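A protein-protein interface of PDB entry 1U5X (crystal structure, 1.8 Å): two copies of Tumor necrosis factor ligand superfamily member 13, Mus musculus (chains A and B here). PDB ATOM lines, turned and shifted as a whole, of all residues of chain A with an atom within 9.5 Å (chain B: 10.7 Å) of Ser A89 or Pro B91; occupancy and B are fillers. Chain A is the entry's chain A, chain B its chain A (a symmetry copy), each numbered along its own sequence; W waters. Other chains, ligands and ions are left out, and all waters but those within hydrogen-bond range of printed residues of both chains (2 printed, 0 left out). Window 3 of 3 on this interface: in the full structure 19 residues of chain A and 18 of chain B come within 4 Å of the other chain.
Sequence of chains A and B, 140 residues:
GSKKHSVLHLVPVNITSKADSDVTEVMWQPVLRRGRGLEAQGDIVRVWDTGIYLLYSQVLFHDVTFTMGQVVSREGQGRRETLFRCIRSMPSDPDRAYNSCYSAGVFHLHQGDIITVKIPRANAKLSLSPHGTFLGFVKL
Thr A67 touches Tyr B98, but with the chains exchanged Tyr A98 does not touch Thr B67 (15.9 Å). Arg A88 touches Asn B99, but with the chains exchanged Asn A99 does not touch Arg B88 (7.5 Å). Ser A89 touches Pro B91, but with the chains exchanged Pro A91 does not touch Ser B89 (9.4 Å). Ser A89 touches Tyr B98, but with the chains exchanged Tyr A98 does not touch Ser B89 (11.0 Å).
The side-chain sulfur of Cys A86 is disulfide-bonded to the side-chain sulfur of Cys A101. The side-chain amide nitrogen (ND2) of Asn A99 is in hydrogen-bond range of the backbone carbonyl oxygen (O) of Ser A89 (3.4 Å). N of Phe B61 sits at hydrogen-bond distance from O of Asn B99 (2.9 Å). The backbone NH (N) of Thr B65 sits at hydrogen-bond distance from the backbone carbonyl oxygen (O) of Pro B91, 2.9 Å away. The backbone carbonyl oxygen of Met B68 sits at hydrogen-bond distance from the backbone NH of Arg B88 (2.7 Å). SD of Met B90 is in hydrogen-bond range of ND2 of Asn B99 (3.4 Å).
Of the 20 printed residues of chain A, 5 touch a printed residue of chain B. Hydrophobic or aromatic side chains of chain A within 4 Å of the printed part of chain B: Ile A87. Of the 20 printed residues of chain B, 7 touch a printed residue of chain A. Printed residues of chain B that touch a printed residue of chain A: Leu B60, Arg B88, Pro B91, Ala B97, Tyr B98, Asn B99 and Ser B100. Among the printed residues, 14 pairs touch across the chains. Among the printed residues, no Asp or Glu carboxylate lies within 4 Å of a Lys or Arg side-chain nitrogen of the other chain.
Thr A67 touches one residue of chain B. Of the printed residues of chain B, Arg A88 touches Arg B88, Tyr B98, Asn B99 and Ser B100. Ser A89 touches just these residues of chain B: Pro B91, Ala B97, Tyr B98 and Asn B99. No residue of chain B comes within 4 Å of Pro A91. Of chain A, only Ser A89 (3.5 Å) comes within 4 Å of Pro B91. No residue of chain A comes within 4 Å of Ser B92. Ala B97 touches one residue of chain A. Of the printed residues of chain A, Ser B100 touches Cys A86, Ile A87 and Arg A88. The nearest printed residue of chain A that does not touch Asn B99 is Thr A67 (6.0 Å).
Tyr B98 touches Thr A67. CD1 of Leu B60 touches CD1 of Ile A87 (3.4 Å). CB of Tyr B98 touches CG2 of Ile A87 (3.98 Å). Asn B99 touches Ile A87 (CA to O, 3.4 Å). C of Arg A88 touches O of Tyr B98, 3.9 Å away. Arg A88 touches Asn B99 (CA to OD1, 3.3 Å). Ser A89 touches Pro B91.
Water W2 lies within hydrogen-bond range of the side-chain hydroxyl of Ser B100 (2.6 Å) and the side-chain sulfur of Cys A86 (3.3 Å). Water W1 lies within hydrogen-bond range of O of Ser A89 (2.7 Å) and OD1 of Asn B99 (2.9 Å).
The side-chain hydroxyl of Ser B100 sits close to the side-chain sulfur of Cys A86 (3.6 Å). N of Ile A87 sits at hydrogen-bond distance from OG of Ser B100. The backbone carbonyl oxygen (O) of Ser B100 is in hydrogen-bond range of the guanidinium group (NH1) of Arg A88, 2.7 Å away. The side-chain hydroxyl (OG) of Ser A89 is in hydrogen-bond range of the backbone NH (N) of Ala B97 (3.5 Å). O of Tyr B98 lies within hydrogen-bond range of OG of Ser A89. The side-chain amide oxygen (OD1) of Asn B99 lies within hydrogen-bond range of the backbone NH (N) of Ser A89 (3.0 Å). The guanidinium group (NH2) of Arg A88 sits close to the guanidinium group (NH2) of Arg B88 (3.2 Å).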
ATOM      1  N   PHE A  61      30.741 -15.686  11.169  1.00  0.00           N
ATOM      2  CA  PHE A  61      31.380 -14.588  11.937  1.00  0.00           C
ATOM      3  C   PHE A  61      31.896 -15.049  13.295  1.00  0.00           C
ATOM      4  O   PHE A  61      31.232 -15.851  13.969  1.00  0.00           O
ATOM      5  CB  PHE A  61      30.360 -13.476  12.158  1.00  0.00           C
ATOM      6  CG  PHE A  61      29.877 -12.831  10.895  1.00  0.00           C
ATOM      7  CD1 PHE A  61      30.566 -11.754  10.329  1.00  0.00           C
ATOM      8  CD2 PHE A  61      28.695 -13.240  10.315  1.00  0.00           C
ATOM      9  CE1 PHE A  61      30.090 -11.143   9.175  1.00  0.00           C
ATOM     10  CE2 PHE A  61      28.225 -12.635   9.180  1.00  0.00           C
ATOM     11  CZ  PHE A  61      28.913 -11.577   8.611  1.00  0.00           C
ATOM     12  N   ASP A  63      33.224 -12.414  15.519  1.00  0.00           N
ATOM     13  CA  ASP A  63      33.319 -11.161  16.266  1.00  0.00           C
ATOM     14  C   ASP A  63      32.510 -11.146  17.550  1.00  0.00           C
ATOM     15  O   ASP A  63      31.364 -11.605  17.594  1.00  0.00           O
ATOM     16  CB  ASP A  63      32.856  -9.977  15.418  1.00  0.00           C
ATOM     17  CG  ASP A  63      33.922  -9.495  14.461  1.00  0.00           C
ATOM     18  OD1 ASP A  63      35.099  -9.470  14.863  1.00  0.00           O
ATOM     19  OD2 ASP A  63      33.690  -9.085  13.310  1.00  0.00           O
ATOM     20  N   VAL A  64      33.119 -10.560  18.572  1.00  0.00           N
ATOM     21  CA  VAL A  64      32.484 -10.335  19.859  1.00  0.00           C
ATOM     22  C   VAL A  64      31.598  -9.072  19.771  1.00  0.00           C
ATOM     23  O   VAL A  64      31.887  -8.158  18.996  1.00  0.00           O
ATOM     24  CB  VAL A  64      33.570 -10.250  20.988  1.00  0.00           C
ATOM     25  CG1 VAL A  64      34.447  -8.980  20.886  1.00  0.00           C
ATOM     26  CG2 VAL A  64      32.957 -10.350  22.373  1.00  0.00           C
ATOM     27  N   THR A  65      30.504  -9.068  20.534  1.00  0.00           N
ATOM     28  CA  THR A  65      29.615  -7.905  20.748  1.00  0.00           C
ATOM     29  C   THR A  65      28.660  -7.418  19.661  1.00  0.00           C
ATOM     30  O   THR A  65      27.445  -7.401  19.872  1.00  0.00           O
ATOM     31  CB  THR A  65      30.418  -6.668  21.226  1.00  0.00           C
ATOM     32  OG1 THR A  65      30.633  -6.768  22.631  1.00  0.00           O
ATOM     33  CG2 THR A  65      29.587  -5.369  21.074  1.00  0.00           C
ATOM     34  N   PHE A  66      29.201  -6.918  18.555  1.00  0.00           N
ATOM     35  CA  PHE A  66      28.411  -6.062  17.687  1.00  0.00           C
ATOM     36  C   PHE A  66      27.621  -6.851  16.665  1.00  0.00           C
ATOM     37  O   PHE A  66      27.945  -8.003  16.344  1.00  0.00           O
ATOM     38  CB  PHE A  66      29.287  -5.034  16.995  1.00  0.00           C
ATOM     39  N   THR A  67      26.585  -6.205  16.147  1.00  0.00           N
ATOM     40  CA  THR A  67      25.771  -6.786  15.087  1.00  0.00           C
ATOM     41  C   THR A  67      26.634  -6.955  13.842  1.00  0.00           C
ATOM     42  O   THR A  67      27.297  -6.001  13.424  1.00  0.00           O
ATOM     43  CB  THR A  67      24.572  -5.864  14.766  1.00  0.00           C
ATOM     44  OG1 THR A  67      23.746  -5.705  15.931  1.00  0.00           O
ATOM     45  CG2 THR A  67      23.660  -6.495  13.724  1.00  0.00           C
ATOM     46  N   MET A  68      26.607  -8.158  13.264  1.00  0.00           N
ATOM     47  CA  MET A  68      27.350  -8.486  12.066  1.00  0.00           C
ATOM     48  C   MET A  68      26.390  -8.884  10.958  1.00  0.00           C
ATOM     49  O   MET A  68      25.293  -9.322  11.216  1.00  0.00           O
ATOM     50  CB  MET A  68      28.291  -9.648  12.330  1.00  0.00           C
ATOM     51  CG  MET A  68      29.361  -9.351  13.384  1.00  0.00           C
ATOM     52  SD  MET A  68      30.325  -7.846  13.079  1.00  0.00           S
ATOM     53  CE  MET A  68      31.139  -8.231  11.487  1.00  0.00           C
ATOM     54  N   GLY A  69      26.830  -8.742   9.724  1.00  0.00           N
ATOM     55  CA  GLY A  69      26.035  -9.168   8.602  1.00  0.00           C
ATOM     56  C   GLY A  69      26.650  -8.770   7.283  1.00  0.00           C
ATOM     57  O   GLY A  69      27.425  -7.824   7.189  1.00  0.00           O
ATOM     58  N   CYS A  86      21.939 -10.126   5.262  1.00  0.00           N
ATOM     59  CA  CYS A  86      21.767 -10.992   6.411  1.00  0.00           C
ATOM     60  C   CYS A  86      22.247 -10.207   7.622  1.00  0.00           C
ATOM     61  O   CYS A  86      23.221  -9.474   7.505  1.00  0.00           O
ATOM     62  CB  CYS A  86      22.596 -12.240   6.186  1.00  0.00           C
ATOM     63  SG  CYS A  86      22.235 -13.482   7.400  1.00  0.00           S
ATOM     64  N   ILE A  87      21.553 -10.292   8.756  1.00  0.00           N
ATOM     65  CA  ILE A  87      21.968  -9.550   9.963  1.00  0.00           C
ATOM     66  C   ILE A  87      21.915 -10.451  11.202  1.00  0.00           C
ATOM     67  O   ILE A  87      20.930 -11.148  11.387  1.00  0.00           O
ATOM     68  CB  ILE A  87      21.066  -8.292  10.197  1.00  0.00           C
ATOM     69  CG1 ILE A  87      20.949  -7.440   8.942  1.00  0.00           C
ATOM     70  CG2 ILE A  87      21.655  -7.437  11.291  1.00  0.00           C
ATOM     71  CD1 ILE A  87      19.750  -6.583   8.957  1.00  0.00           C
ATOM     72  N   ARG A  88      22.937 -10.403  12.067  1.00  0.00           N
ATOM     73  CA  ARG A  88      23.010 -11.241  13.275  1.00  0.00           C
ATOM     74  C   ARG A  88      23.624 -10.495  14.421  1.00  0.00           C
ATOM     75  O   ARG A  88      24.749 -10.056  14.291  1.00  0.00           O
ATOM     76  CB  ARG A  88      23.930 -12.448  13.067  1.00  0.00           C
ATOM     77  CG  ARG A  88      23.385 -13.499  12.210  1.00  0.00           C
ATOM     78  CD  ARG A  88      22.889 -14.740  12.928  1.00  0.00           C
ATOM     79  NE  ARG A  88      22.118 -15.518  11.980  1.00  0.00           N
ATOM     80  CZ  ARG A  88      21.026 -15.093  11.346  1.00  0.00           C
ATOM     81  NH1 ARG A  88      20.501 -13.895  11.584  1.00  0.00           N
ATOM     82  NH2 ARG A  88      20.442 -15.885  10.458  1.00  0.00           N
ATOM     83  N   SER A  89      22.925 -10.405  15.549  1.00  0.00           N
ATOM     84  CA  SER A  89      23.547  -9.939  16.787  1.00  0.00           C
ATOM     85  C   SER A  89      24.512 -11.016  17.300  1.00  0.00           C
ATOM     86  O   SER A  89      24.277 -12.232  17.138  1.00  0.00           O
ATOM     87  CB  SER A  89      22.491  -9.624  17.831  1.00  0.00           C
ATOM     88  OG  SER A  89      21.630  -8.609  17.357  1.00  0.00           O
ATOM     89  N   MET A  90      25.623 -10.558  17.869  1.00  0.00           N
ATOM     90  CA  MET A  90      26.659 -11.435  18.385  1.00  0.00           C
ATOM     91  C   MET A  90      26.673 -11.335  19.904  1.00  0.00           C
ATOM     92  O   MET A  90      26.446 -10.245  20.452  1.00  0.00           O
ATOM     93  CB  MET A  90      28.025 -11.031  17.808  1.00  0.00           C
ATOM     94  CG  MET A  90      28.138 -11.136  16.288  1.00  0.00           C
ATOM     95  SD  MET A  90      27.876 -12.807  15.637  1.00  0.00           S
ATOM     96  CE  MET A  90      29.097 -13.801  16.662  1.00  0.00           C
ATOM     97  N   PRO A  91      26.909 -12.458  20.594  1.00  0.00           N
ATOM     98  CA  PRO A  91      27.080 -12.447  22.052  1.00  0.00           C
ATOM     99  C   PRO A  91      28.235 -11.559  22.497  1.00  0.00           C
ATOM    100  O   PRO A  91      29.187 -11.369  21.745  1.00  0.00           O
ATOM    101  CB  PRO A  91      27.425 -13.908  22.383  1.00  0.00           C
ATOM    102  CG  PRO A  91      26.891 -14.698  21.268  1.00  0.00           C
ATOM    103  CD  PRO A  91      26.997 -13.827  20.053  1.00  0.00           C
ATOM    104  N   SER A  92      28.147 -11.045  23.715  1.00  0.00           N
ATOM    105  CA  SER A  92      29.216 -10.225  24.277  1.00  0.00           C
ATOM    106  C   SER A  92      30.400 -11.078  24.769  1.00  0.00           C
ATOM    107  O   SER A  92      31.511 -10.568  24.898  1.00  0.00           O
ATOM    108  CB  SER A  92      28.676  -9.310  25.382  1.00  0.00           C
ATOM    109  OG  SER A  92      27.932 -10.025  26.353  1.00  0.00           O
ATOM    110  N   ALA A  97      29.703 -15.606  20.536  1.00  0.00           N
ATOM    111  CA  ALA A  97      31.024 -15.686  19.941  1.00  0.00           C
ATOM    112  C   ALA A  97      31.001 -16.165  18.480  1.00  0.00           C
ATOM    113  O   ALA A  97      31.892 -15.838  17.690  1.00  0.00           O
ATOM    114  CB  ALA A  97      31.891 -16.593  20.783  1.00  0.00           C
ATOM    115  N   TYR A  98      29.990 -16.952  18.117  1.00  0.00           N
ATOM    116  CA  TYR A  98      29.997 -17.629  16.839  1.00  0.00           C
ATOM    117  C   TYR A  98      28.613 -17.654  16.240  1.00  0.00           C
ATOM    118  O   TYR A  98      27.625 -17.945  16.939  1.00  0.00           O
ATOM    119  CB  TYR A  98      30.473 -19.064  16.992  1.00  0.00           C
ATOM    120  CG  TYR A  98      31.833 -19.211  17.608  1.00  0.00           C
ATOM    121  CD1 TYR A  98      31.981 -19.268  18.987  1.00  0.00           C
ATOM    122  CD2 TYR A  98      32.975 -19.309  16.818  1.00  0.00           C
ATOM    123  CE1 TYR A  98      33.228 -19.406  19.558  1.00  0.00           C
ATOM    124  CE2 TYR A  98      34.225 -19.460  17.378  1.00  0.00           C
ATOM    125  CZ  TYR A  98      34.347 -19.503  18.751  1.00  0.00           C
ATOM    126  OH  TYR A  98      35.581 -19.652  19.332  1.00  0.00           O
ATOM    127  N   ASN A  99      28.542 -17.335  14.956  1.00  0.00           N
ATOM    128  CA  ASN A  99      27.264 -17.319  14.240  1.00  0.00           C
ATOM    129  C   ASN A  99      27.443 -17.288  12.734  1.00  0.00           C
ATOM    130  O   ASN A  99      28.143 -16.427  12.222  1.00  0.00           O
ATOM    131  CB  ASN A  99      26.465 -16.063  14.636  1.00  0.00           C
ATOM    132  CG  ASN A  99      25.698 -16.216  15.938  1.00  0.00           C
ATOM    133  OD1 ASN A  99      24.934 -17.157  16.119  1.00  0.00           O
ATOM    134  ND2 ASN A  99      25.867 -15.243  16.847  1.00  0.00           N
ATOM    135  N   SER A 100      26.771 -18.197  12.018  1.00  0.00           N
ATOM    136  CA  SER A 100      26.674 -18.119  10.579  1.00  0.00           C
ATOM    137  C   SER A 100      25.455 -17.258  10.241  1.00  0.00           C
ATOM    138  O   SER A 100      24.461 -17.230  10.963  1.00  0.00           O
ATOM    139  CB  SER A 100      26.582 -19.528   9.928  1.00  0.00           C
ATOM    140  OG  SER A 100      25.516 -20.295  10.445  1.00  0.00           O
ATOM    141  N   CYS A 101      25.551 -16.528   9.149  1.00  0.00           N
ATOM    142  CA  CYS A 101      24.460 -15.718   8.655  1.00  0.00           C
ATOM    143  C   CYS A 101      24.227 -16.145   7.226  1.00  0.00           C
ATOM    144  O   CYS A 101      25.061 -15.923   6.370  1.00  0.00           O
ATOM    145  CB  CYS A 101      24.839 -14.239   8.755  1.00  0.00           C
ATOM    146  SG  CYS A 101      23.446 -13.157   8.978  1.00  0.00           S
ATOM    147  N   LEU B  60      13.261  -9.587   8.752  1.00  0.00           N
ATOM    148  CA  LEU B  60      14.235  -8.835   9.520  1.00  0.00           C
ATOM    149  C   LEU B  60      13.573  -8.259  10.775  1.00  0.00           C
ATOM    150  O   LEU B  60      12.654  -7.462  10.673  1.00  0.00           O
ATOM    151  CB  LEU B  60      14.812  -7.717   8.654  1.00  0.00           C
ATOM    152  CG  LEU B  60      15.672  -6.674   9.355  1.00  0.00           C
ATOM    153  CD1 LEU B  60      16.735  -7.393  10.179  1.00  0.00           C
ATOM    154  CD2 LEU B  60      16.282  -5.697   8.300  1.00  0.00           C
ATOM    155  N   PHE B  61      14.006  -8.698  11.948  1.00  0.00           N
ATOM    156  CA  PHE B  61      13.351  -8.264  13.208  1.00  0.00           C
ATOM    157  C   PHE B  61      14.179  -7.237  13.972  1.00  0.00           C
ATOM    158  O   PHE B  61      15.411  -7.356  14.029  1.00  0.00           O
ATOM    159  CB  PHE B  61      13.138  -9.479  14.103  1.00  0.00           C
ATOM    160  CG  PHE B  61      12.217 -10.509  13.526  1.00  0.00           C
ATOM    161  CD1 PHE B  61      10.834 -10.427  13.722  1.00  0.00           C
ATOM    162  CD2 PHE B  61      12.726 -11.602  12.859  1.00  0.00           C
ATOM    163  CE1 PHE B  61       9.992 -11.406  13.209  1.00  0.00           C
ATOM    164  CE2 PHE B  61      11.896 -12.568  12.357  1.00  0.00           C
ATOM    165  CZ  PHE B  61      10.526 -12.481  12.540  1.00  0.00           C
ATOM    166  N   HIS B  62      13.501  -6.281  14.625  1.00  0.00           N
ATOM    167  CA  HIS B  62      14.156  -5.251  15.444  1.00  0.00           C
ATOM    168  C   HIS B  62      13.733  -5.289  16.924  1.00  0.00           C
ATOM    169  O   HIS B  62      14.182  -4.459  17.711  1.00  0.00           O
ATOM    170  CB  HIS B  62      13.890  -3.857  14.849  1.00  0.00           C
ATOM    171  N   ASP B  63      12.904  -6.261  17.299  1.00  0.00           N
ATOM    172  CA  ASP B  63      12.373  -6.370  18.657  1.00  0.00           C
ATOM    173  C   ASP B  63      13.418  -6.707  19.704  1.00  0.00           C
ATOM    174  O   ASP B  63      14.285  -7.562  19.495  1.00  0.00           O
ATOM    175  CB  ASP B  63      11.281  -7.437  18.738  1.00  0.00           C
ATOM    176  CG  ASP B  63       9.942  -6.938  18.247  1.00  0.00           C
ATOM    177  OD1 ASP B  63       9.611  -5.774  18.536  1.00  0.00           O
ATOM    178  OD2 ASP B  63       9.134  -7.631  17.603  1.00  0.00           O
ATOM    179  N   VAL B  64      13.278  -6.051  20.847  1.00  0.00           N
ATOM    180  CA  VAL B  64      14.098  -6.303  22.020  1.00  0.00           C
ATOM    181  C   VAL B  64      13.551  -7.543  22.762  1.00  0.00           C
ATOM    182  O   VAL B  64      12.352  -7.826  22.707  1.00  0.00           O
ATOM    183  CB  VAL B  64      14.157  -5.019  22.921  1.00  0.00           C
ATOM    184  CG1 VAL B  64      12.803  -4.694  23.595  1.00  0.00           C
ATOM    185  CG2 VAL B  64      15.251  -5.114  23.970  1.00  0.00           C
ATOM    186  N   THR B  65      14.452  -8.289  23.402  1.00  0.00           N
ATOM    187  CA  THR B  65      14.141  -9.407  24.319  1.00  0.00           C
ATOM    188  C   THR B  65      13.638 -10.751  23.799  1.00  0.00           C
ATOM    189  O   THR B  65      14.288 -11.777  24.019  1.00  0.00           O
ATOM    190  CB  THR B  65      13.156  -8.960  25.431  1.00  0.00           C
ATOM    191  OG1 THR B  65      13.887  -8.309  26.465  1.00  0.00           O
ATOM    192  CG2 THR B  65      12.525 -10.183  26.142  1.00  0.00           C
ATOM    193  N   PHE B  66      12.443 -10.772  23.220  1.00  0.00           N
ATOM    194  CA  PHE B  66      11.722 -12.027  23.094  1.00  0.00           C
ATOM    195  C   PHE B  66      12.088 -12.776  21.831  1.00  0.00           C
ATOM    196  O   PHE B  66      12.589 -12.199  20.857  1.00  0.00           O
ATOM    197  CB  PHE B  66      10.222 -11.799  23.155  1.00  0.00           C
ATOM    198  N   THR B  67      11.816 -14.074  21.860  1.00  0.00           N
ATOM    199  CA  THR B  67      12.025 -14.927  20.696  1.00  0.00           C
ATOM    200  C   THR B  67      11.085 -14.478  19.584  1.00  0.00           C
ATOM    201  O   THR B  67       9.882 -14.333  19.821  1.00  0.00           O
ATOM    202  CB  THR B  67      11.736 -16.403  21.055  1.00  0.00           C
ATOM    203  OG1 THR B  67      12.623 -16.840  22.098  1.00  0.00           O
ATOM    204  CG2 THR B  67      12.033 -17.321  19.879  1.00  0.00           C
ATOM    205  N   MET B  68      11.641 -14.275  18.387  1.00  0.00           N
ATOM    206  CA  MET B  68      10.894 -13.864  17.218  1.00  0.00           C
ATOM    207  C   MET B  68      11.013 -14.923  16.135  1.00  0.00           C
ATOM    208  O   MET B  68      11.958 -15.677  16.105  1.00  0.00           O
ATOM    209  CB  MET B  68      11.439 -12.556  16.675  1.00  0.00           C
ATOM    210  CG  MET B  68      11.314 -11.381  17.649  1.00  0.00           C
ATOM    211  SD  MET B  68       9.644 -11.118  18.304  1.00  0.00           S
ATOM    212  CE  MET B  68       8.693 -10.745  16.787  1.00  0.00           C
ATOM    213  N   ARG B  88      14.247 -17.158  16.189  1.00  0.00           N
ATOM    214  CA  ARG B  88      15.462 -16.446  16.618  1.00  0.00           C
ATOM    215  C   ARG B  88      15.271 -15.801  17.958  1.00  0.00           C
ATOM    216  O   ARG B  88      14.383 -14.984  18.087  1.00  0.00           O
ATOM    217  CB  ARG B  88      15.794 -15.283  15.677  1.00  0.00           C
ATOM    218  CG  ARG B  88      16.325 -15.678  14.374  1.00  0.00           C
ATOM    219  CD  ARG B  88      17.819 -15.486  14.189  1.00  0.00           C
ATOM    220  NE  ARG B  88      18.209 -16.201  12.991  1.00  0.00           N
ATOM    221  CZ  ARG B  88      18.057 -17.509  12.793  1.00  0.00           C
ATOM    222  NH1 ARG B  88      17.569 -18.307  13.739  1.00  0.00           N
ATOM    223  NH2 ARG B  88      18.405 -18.034  11.627  1.00  0.00           N
ATOM    224  N   SER B  89      16.131 -16.113  18.924  1.00  0.00           N
ATOM    225  CA  SER B  89      16.186 -15.339  20.163  1.00  0.00           C
ATOM    226  C   SER B  89      16.795 -13.961  19.868  1.00  0.00           C
ATOM    227  O   SER B  89      17.679 -13.812  18.998  1.00  0.00           O
ATOM    228  CB  SER B  89      17.002 -16.069  21.215  1.00  0.00           C
ATOM    229  OG  SER B  89      16.412 -17.322  21.500  1.00  0.00           O
ATOM    230  N   MET B  90      16.275 -12.951  20.558  1.00  0.00           N
ATOM    231  CA  MET B  90      16.710 -11.577  20.386  1.00  0.00           C
ATOM    232  C   MET B  90      17.452 -11.138  21.641  1.00  0.00           C
ATOM    233  O   MET B  90      17.074 -11.539  22.753  1.00  0.00           O
ATOM    234  CB  MET B  90      15.497 -10.669  20.135  1.00  0.00           C
ATOM    235  CG  MET B  90      14.701 -10.994  18.871  1.00  0.00           C
ATOM    236  SD  MET B  90      15.656 -10.865  17.337  1.00  0.00           S
ATOM    237  CE  MET B  90      16.366  -9.132  17.486  1.00  0.00           C
ATOM    238  N   PRO B  91      18.517 -10.341  21.482  1.00  0.00           N
ATOM    239  CA  PRO B  91      19.218  -9.750  22.628  1.00  0.00           C
ATOM    240  C   PRO B  91      18.306  -8.883  23.485  1.00  0.00           C
ATOM    241  O   PRO B  91      17.335  -8.325  22.979  1.00  0.00           O
ATOM    242  CB  PRO B  91      20.281  -8.853  21.973  1.00  0.00           C
ATOM    243  CG  PRO B  91      20.481  -9.402  20.628  1.00  0.00           C
ATOM    244  CD  PRO B  91      19.160  -9.968  20.208  1.00  0.00           C
ATOM    245  N   SER B  92      18.636  -8.765  24.763  1.00  0.00           N
ATOM    246  CA  SER B  92      17.874  -7.915  25.674  1.00  0.00           C
ATOM    247  C   SER B  92      18.213  -6.424  25.492  1.00  0.00           C
ATOM    248  O   SER B  92      17.419  -5.565  25.869  1.00  0.00           O
ATOM    249  CB  SER B  92      18.062  -8.369  27.126  1.00  0.00           C
ATOM    250  OG  SER B  92      19.429  -8.499  27.473  1.00  0.00           O
ATOM    251  N   ASP B  93      19.374  -6.129  24.901  1.00  0.00           N
ATOM    252  CA  ASP B  93      19.803  -4.754  24.594  1.00  0.00           C
ATOM    253  C   ASP B  93      18.647  -3.832  24.189  1.00  0.00           C
ATOM    254  O   ASP B  93      18.324  -3.706  23.001  1.00  0.00           O
ATOM    255  CB  ASP B  93      20.846  -4.772  23.476  1.00  0.00           C
ATOM    256  N   ALA B  97      19.466  -6.811  19.394  1.00  0.00           N
ATOM    257  CA  ALA B  97      18.607  -5.787  18.831  1.00  0.00           C
ATOM    258  C   ALA B  97      18.171  -6.089  17.388  1.00  0.00           C
ATOM    259  O   ALA B  97      17.111  -5.644  16.938  1.00  0.00           O
ATOM    260  CB  ALA B  97      19.316  -4.454  18.902  1.00  0.00           C
ATOM    261  N   TYR B  98      18.991  -6.837  16.652  1.00  0.00           N
ATOM    262  CA  TYR B  98      18.781  -6.992  15.229  1.00  0.00           C
ATOM    263  C   TYR B  98      19.099  -8.400  14.791  1.00  0.00           C
ATOM    264  O   TYR B  98      20.128  -8.972  15.196  1.00  0.00           O
ATOM    265  CB  TYR B  98      19.669  -6.039  14.446  1.00  0.00           C
ATOM    266  CG  TYR B  98      19.493  -4.591  14.793  1.00  0.00           C
ATOM    267  CD1 TYR B  98      20.211  -4.021  15.835  1.00  0.00           C
ATOM    268  CD2 TYR B  98      18.623  -3.779  14.072  1.00  0.00           C
ATOM    269  CE1 TYR B  98      20.054  -2.690  16.156  1.00  0.00           C
ATOM    270  CE2 TYR B  98      18.468  -2.443  14.375  1.00  0.00           C
ATOM    271  CZ  TYR B  98      19.185  -1.903  15.423  1.00  0.00           C
ATOM    272  OH  TYR B  98      19.048  -0.577  15.743  1.00  0.00           O
ATOM    273  N   ASN B  99      18.212  -8.959  13.983  1.00  0.00           N
ATOM    274  CA  ASN B  99      18.390 -10.321  13.474  1.00  0.00           C
ATOM    275  C   ASN B  99      17.475 -10.629  12.304  1.00  0.00           C
ATOM    276  O   ASN B  99      16.271 -10.448  12.409  1.00  0.00           O
ATOM    277  CB  ASN B  99      18.070 -11.336  14.589  1.00  0.00           C
ATOM    278  CG  ASN B  99      19.227 -11.573  15.545  1.00  0.00           C
ATOM    279  OD1 ASN B  99      20.338 -11.885  15.132  1.00  0.00           O
ATOM    280  ND2 ASN B  99      18.947 -11.473  16.854  1.00  0.00           N
ATOM    281  N   SER B 100      18.039 -11.140  11.204  1.00  0.00           N
ATOM    282  CA  SER B 100      17.251 -11.690  10.125  1.00  0.00           C
ATOM    283  C   SER B 100      17.006 -13.168  10.433  1.00  0.00           C
ATOM    284  O   SER B 100      17.823 -13.846  11.052  1.00  0.00           O
ATOM    285  CB  SER B 100      17.944 -11.497   8.746  1.00  0.00           C
ATOM    286  OG  SER B 100      19.249 -12.034   8.715  1.00  0.00           O
ATOM    287  N   CYS B 101      15.855 -13.658  10.023  1.00  0.00           N
ATOM    288  CA  CYS B 101      15.503 -15.053  10.173  1.00  0.00           C
ATOM    289  C   CYS B 101      15.141 -15.550   8.794  1.00  0.00           C
ATOM    290  O   CYS B 101      14.147 -15.140   8.229  1.00  0.00           O
ATOM    291  CB  CYS B 101      14.334 -15.179  11.151  1.00  0.00           C
ATOM    292  SG  CYS B 101      14.312 -16.717  12.043  1.00  0.00           S
HETATM  293  O   HOH W   1      22.148 -13.755  16.414  1.00  0.00           O
HETATM  294  O   HOH W   2      18.975 -14.219   7.256  1.00  0.00           O
